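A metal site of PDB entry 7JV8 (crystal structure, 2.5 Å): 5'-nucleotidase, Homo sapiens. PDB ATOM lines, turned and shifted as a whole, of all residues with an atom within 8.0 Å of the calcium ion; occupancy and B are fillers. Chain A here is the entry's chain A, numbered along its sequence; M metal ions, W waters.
O of Asn 191 is bound to the calcium ion, 2.2 Å away.
Water W2 binds the calcium ion (2.3 Å).
O of Gly 276 is bound to the calcium ion (2.4 Å).
OD2 of Asp 215 binds the calcium ion (2.4 Å).
The calcium ion is bound by OD1 of Asp 215, 2.4 Å away.
Water W1 binds the calcium ion, 2.5 Å away.
Within 4 Å of the calcium ion: Asn 191, Asp 215 and Gly 276.
The backbone NH of Gly 276 is in hydrogen-bond range of the side-chain carboxylate of Asp 273 (3.1 Å).
The side-chain amide oxygen (OD1) of Asn 191 sits at hydrogen-bond distance from the side-chain amino group (NZ) of Lys 192 (2.8 Å).
The backbone NH of Asp 215 sits at hydrogen-bond distance from the backbone carbonyl oxygen of Ile 193.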
ATOM      1  N   VAL A 182      15.294  20.664 -39.389  1.00  0.00           N
ATOM      2  CA  VAL A 182      15.385  20.126 -38.012  1.00  0.00           C
ATOM      3  C   VAL A 182      16.125  18.781 -37.981  1.00  0.00           C
ATOM      4  O   VAL A 182      16.898  18.514 -37.045  1.00  0.00           O
ATOM      5  CB  VAL A 182      13.976  20.043 -37.335  1.00  0.00           C
ATOM      6  CG1 VAL A 182      14.037  19.400 -35.958  1.00  0.00           C
ATOM      7  CG2 VAL A 182      13.390  21.443 -37.167  1.00  0.00           C
ATOM      8  N   LYS A 186      19.863  17.778 -36.125  1.00  0.00           N
ATOM      9  CA  LYS A 186      20.154  16.527 -35.395  1.00  0.00           C
ATOM     10  C   LYS A 186      21.462  15.863 -35.859  1.00  0.00           C
ATOM     11  O   LYS A 186      22.236  15.400 -35.017  1.00  0.00           O
ATOM     12  CB  LYS A 186      18.984  15.535 -35.483  1.00  0.00           C
ATOM     13  CG  LYS A 186      18.988  14.532 -34.328  1.00  0.00           C
ATOM     14  CD  LYS A 186      18.003  13.387 -34.572  1.00  0.00           C
ATOM     15  CE  LYS A 186      18.058  12.369 -33.447  1.00  0.00           C
ATOM     16  N   VAL A 190      22.976  18.958 -32.576  1.00  0.00           N
ATOM     17  CA  VAL A 190      22.178  20.021 -31.963  1.00  0.00           C
ATOM     18  C   VAL A 190      20.936  19.286 -31.500  1.00  0.00           C
ATOM     19  O   VAL A 190      20.126  18.848 -32.328  1.00  0.00           O
ATOM     20  CB  VAL A 190      21.846  21.161 -32.959  1.00  0.00           C
ATOM     21  CG1 VAL A 190      21.091  22.281 -32.260  1.00  0.00           C
ATOM     22  CG2 VAL A 190      23.130  21.702 -33.581  1.00  0.00           C
ATOM     23  N   ASN A 191      20.823  19.114 -30.181  1.00  0.00           N
ATOM     24  CA  ASN A 191      19.670  18.459 -29.533  1.00  0.00           C
ATOM     25  C   ASN A 191      18.632  19.424 -28.903  1.00  0.00           C
ATOM     26  O   ASN A 191      17.542  18.984 -28.496  1.00  0.00           O
ATOM     27  CB  ASN A 191      20.164  17.397 -28.529  1.00  0.00           C
ATOM     28  CG  ASN A 191      21.066  17.941 -27.408  1.00  0.00           C
ATOM     29  OD1 ASN A 191      20.815  18.993 -26.816  1.00  0.00           O
ATOM     30  ND2 ASN A 191      22.101  17.181 -27.075  1.00  0.00           N
ATOM     31  N   LYS A 192      19.017  20.699 -28.753  1.00  0.00           N
ATOM     32  CA  LYS A 192      18.134  21.782 -28.314  1.00  0.00           C
ATOM     33  C   LYS A 192      17.752  22.620 -29.528  1.00  0.00           C
ATOM     34  O   LYS A 192      18.614  23.292 -30.103  1.00  0.00           O
ATOM     35  CB  LYS A 192      18.827  22.615 -27.241  1.00  0.00           C
ATOM     36  CG  LYS A 192      18.931  21.870 -25.913  1.00  0.00           C
ATOM     37  CD  LYS A 192      19.932  22.487 -24.970  1.00  0.00           C
ATOM     38  CE  LYS A 192      21.360  22.055 -25.260  1.00  0.00           C
ATOM     39  NZ  LYS A 192      21.634  20.672 -24.787  1.00  0.00           N
ATOM     40  N   ILE A 193      16.468  22.554 -29.933  1.00  0.00           N
ATOM     41  CA  ILE A 193      15.968  23.152 -31.172  1.00  0.00           C
ATOM     42  C   ILE A 193      14.733  24.018 -30.875  1.00  0.00           C
ATOM     43  O   ILE A 193      13.698  23.492 -30.429  1.00  0.00           O
ATOM     44  CB  ILE A 193      15.664  22.064 -32.237  1.00  0.00           C
ATOM     45  CG1 ILE A 193      16.980  21.419 -32.693  1.00  0.00           C
ATOM     46  CG2 ILE A 193      14.920  22.652 -33.448  1.00  0.00           C
ATOM     47  CD1 ILE A 193      16.800  20.109 -33.411  1.00  0.00           C
ATOM     48  N   ILE A 194      14.847  25.318 -31.149  1.00  0.00           N
ATOM     49  CA  ILE A 194      13.743  26.279 -31.019  1.00  0.00           C
ATOM     50  C   ILE A 194      13.195  26.546 -32.427  1.00  0.00           C
ATOM     51  O   ILE A 194      13.976  26.780 -33.364  1.00  0.00           O
ATOM     52  CB  ILE A 194      14.188  27.610 -30.382  1.00  0.00           C
ATOM     53  CG1 ILE A 194      14.892  27.375 -29.032  1.00  0.00           C
ATOM     54  CG2 ILE A 194      12.983  28.518 -30.180  1.00  0.00           C
ATOM     55  CD1 ILE A 194      15.726  28.550 -28.584  1.00  0.00           C
ATOM     56  N   ARG A 212       9.125  16.713 -35.800  1.00  0.00           N
ATOM     57  CA  ARG A 212       9.934  15.936 -34.839  1.00  0.00           C
ATOM     58  C   ARG A 212      11.298  16.599 -34.627  1.00  0.00           C
ATOM     59  O   ARG A 212      11.895  17.091 -35.583  1.00  0.00           O
ATOM     60  CB  ARG A 212      10.141  14.483 -35.311  1.00  0.00           C
ATOM     61  CG  ARG A 212       8.875  13.660 -35.504  1.00  0.00           C
ATOM     62  CD  ARG A 212       9.161  12.336 -36.231  1.00  0.00           C
ATOM     63  NE  ARG A 212       9.832  12.527 -37.533  1.00  0.00           N
ATOM     64  CZ  ARG A 212       9.264  12.942 -38.673  1.00  0.00           C
ATOM     65  NH1 ARG A 212       7.959  13.233 -38.752  1.00  0.00           N
ATOM     66  NH2 ARG A 212      10.023  13.077 -39.775  1.00  0.00           N
ATOM     67  N   GLY A 213      11.755  16.613 -33.375  1.00  0.00           N
ATOM     68  CA  GLY A 213      12.939  17.360 -32.953  1.00  0.00           C
ATOM     69  C   GLY A 213      12.703  18.722 -32.311  1.00  0.00           C
ATOM     70  O   GLY A 213      13.572  19.194 -31.567  1.00  0.00           O
ATOM     71  N   VAL A 214      11.566  19.378 -32.596  1.00  0.00           N
ATOM     72  CA  VAL A 214      11.291  20.744 -32.115  1.00  0.00           C
ATOM     73  C   VAL A 214      10.930  20.693 -30.635  1.00  0.00           C
ATOM     74  O   VAL A 214       9.955  20.049 -30.258  1.00  0.00           O
ATOM     75  CB  VAL A 214      10.176  21.450 -32.930  1.00  0.00           C
ATOM     76  CG1 VAL A 214       9.802  22.816 -32.354  1.00  0.00           C
ATOM     77  CG2 VAL A 214      10.600  21.611 -34.384  1.00  0.00           C
ATOM     78  N   ASP A 215      11.714  21.389 -29.821  1.00  0.00           N
ATOM     79  CA  ASP A 215      11.582  21.387 -28.368  1.00  0.00           C
ATOM     80  C   ASP A 215      10.679  22.511 -27.851  1.00  0.00           C
ATOM     81  O   ASP A 215       9.974  22.300 -26.874  1.00  0.00           O
ATOM     82  CB  ASP A 215      12.977  21.454 -27.722  1.00  0.00           C
ATOM     83  CG  ASP A 215      13.838  20.236 -28.049  1.00  0.00           C
ATOM     84  OD1 ASP A 215      13.355  19.102 -27.862  1.00  0.00           O
ATOM     85  OD2 ASP A 215      15.012  20.416 -28.472  1.00  0.00           O
ATOM     86  N   VAL A 216      10.745  23.689 -28.484  1.00  0.00           N
ATOM     87  CA  VAL A 216       9.917  24.864 -28.134  1.00  0.00           C
ATOM     88  C   VAL A 216       9.499  25.571 -29.429  1.00  0.00           C
ATOM     89  O   VAL A 216      10.276  25.612 -30.397  1.00  0.00           O
ATOM     90  CB  VAL A 216      10.696  25.898 -27.270  1.00  0.00           C
ATOM     91  CG1 VAL A 216       9.782  27.003 -26.734  1.00  0.00           C
ATOM     92  CG2 VAL A 216      11.409  25.218 -26.095  1.00  0.00           C
ATOM     93  N   ARG A 251       6.047  13.742 -26.813  1.00  0.00           N
ATOM     94  CA  ARG A 251       6.757  14.779 -26.036  1.00  0.00           C
ATOM     95  C   ARG A 251       5.850  15.971 -25.702  1.00  0.00           C
ATOM     96  O   ARG A 251       4.937  16.288 -26.453  1.00  0.00           O
ATOM     97  CB  ARG A 251       7.993  15.239 -26.803  1.00  0.00           C
ATOM     98  CG  ARG A 251       9.034  14.146 -26.968  1.00  0.00           C
ATOM     99  CD  ARG A 251      10.246  14.569 -27.790  1.00  0.00           C
ATOM    100  NE  ARG A 251       9.883  14.848 -29.197  1.00  0.00           N
ATOM    101  CZ  ARG A 251       9.602  16.044 -29.743  1.00  0.00           C
ATOM    102  NH1 ARG A 251       9.618  17.183 -29.037  1.00  0.00           N
ATOM    103  NH2 ARG A 251       9.285  16.100 -31.039  1.00  0.00           N
ATOM    104  N   PHE A 272      16.355  21.622 -19.651  1.00  0.00           N
ATOM    105  CA  PHE A 272      16.706  20.530 -20.554  1.00  0.00           C
ATOM    106  C   PHE A 272      17.526  19.462 -19.811  1.00  0.00           C
ATOM    107  O   PHE A 272      18.256  19.785 -18.869  1.00  0.00           O
ATOM    108  CB  PHE A 272      17.560  21.021 -21.729  1.00  0.00           C
ATOM    109  CG  PHE A 272      16.812  21.843 -22.731  1.00  0.00           C
ATOM    110  CD1 PHE A 272      15.980  21.248 -23.689  1.00  0.00           C
ATOM    111  CD2 PHE A 272      16.977  23.227 -22.759  1.00  0.00           C
ATOM    112  CE1 PHE A 272      15.303  22.022 -24.635  1.00  0.00           C
ATOM    113  CE2 PHE A 272      16.317  24.010 -23.717  1.00  0.00           C
ATOM    114  CZ  PHE A 272      15.478  23.406 -24.641  1.00  0.00           C
ATOM    115  N   ASP A 273      17.391  18.205 -20.258  1.00  0.00           N
ATOM    116  CA  ASP A 273      18.337  17.137 -19.891  1.00  0.00           C
ATOM    117  C   ASP A 273      19.542  17.141 -20.838  1.00  0.00           C
ATOM    118  O   ASP A 273      19.583  17.936 -21.790  1.00  0.00           O
ATOM    119  CB  ASP A 273      17.652  15.739 -19.789  1.00  0.00           C
ATOM    120  CG  ASP A 273      17.155  15.176 -21.134  1.00  0.00           C
ATOM    121  OD1 ASP A 273      17.437  15.727 -22.239  1.00  0.00           O
ATOM    122  OD2 ASP A 273      16.431  14.164 -21.063  1.00  0.00           O
ATOM    123  N   ARG A 275      20.424  15.074 -23.194  1.00  0.00           N
ATOM    124  CA  ARG A 275      20.007  14.753 -24.583  1.00  0.00           C
ATOM    125  C   ARG A 275      19.062  15.811 -25.242  1.00  0.00           C
ATOM    126  O   ARG A 275      18.477  15.532 -26.300  1.00  0.00           O
ATOM    127  CB  ARG A 275      19.336  13.344 -24.673  1.00  0.00           C
ATOM    128  CG  ARG A 275      20.093  12.147 -24.070  1.00  0.00           C
ATOM    129  CD  ARG A 275      19.340  11.519 -22.896  1.00  0.00           C
ATOM    130  NE  ARG A 275      18.461  10.418 -23.311  1.00  0.00           N
ATOM    131  CZ  ARG A 275      17.436   9.917 -22.613  1.00  0.00           C
ATOM    132  NH1 ARG A 275      17.083  10.388 -21.417  1.00  0.00           N
ATOM    133  NH2 ARG A 275      16.741   8.894 -23.131  1.00  0.00           N
ATOM    134  N   GLY A 276      18.906  16.988 -24.633  1.00  0.00           N
ATOM    135  CA  GLY A 276      18.084  18.063 -25.199  1.00  0.00           C
ATOM    136  C   GLY A 276      16.584  17.847 -25.187  1.00  0.00           C
ATOM    137  O   GLY A 276      15.893  18.486 -25.983  1.00  0.00           O
ATOM    138  N   ASN A 277      16.082  16.992 -24.299  1.00  0.00           N
ATOM    139  CA  ASN A 277      14.641  16.798 -24.087  1.00  0.00           C
ATOM    140  C   ASN A 277      14.201  17.790 -23.014  1.00  0.00           C
ATOM    141  O   ASN A 277      14.925  18.017 -22.034  1.00  0.00           O
ATOM    142  CB  ASN A 277      14.322  15.379 -23.593  1.00  0.00           C
ATOM    143  CG  ASN A 277      14.803  14.290 -24.537  1.00  0.00           C
ATOM    144  OD1 ASN A 277      14.608  14.381 -25.754  1.00  0.00           O
ATOM    145  ND2 ASN A 277      15.414  13.240 -23.982  1.00  0.00           N
ATOM    146  N   VAL A 278      12.998  18.357 -23.197  1.00  0.00           N
ATOM    147  CA  VAL A 278      12.422  19.301 -22.242  1.00  0.00           C
ATOM    148  C   VAL A 278      11.925  18.521 -21.022  1.00  0.00           C
ATOM    149  O   VAL A 278      10.992  17.726 -21.153  1.00  0.00           O
ATOM    150  CB  VAL A 278      11.250  20.112 -22.874  1.00  0.00           C
ATOM    151  CG1 VAL A 278      10.535  20.991 -21.853  1.00  0.00           C
ATOM    152  CG2 VAL A 278      11.776  20.988 -24.007  1.00  0.00           C
HETATM  153 CA    CA M   1      15.518  18.030 -28.271  1.00  0.00          CA
HETATM  154  O   HOH W   1      13.717  16.356 -28.249  1.00  0.00           O
HETATM  155  O   HOH W   2      15.753  18.004 -30.567  1.00  0.00           O
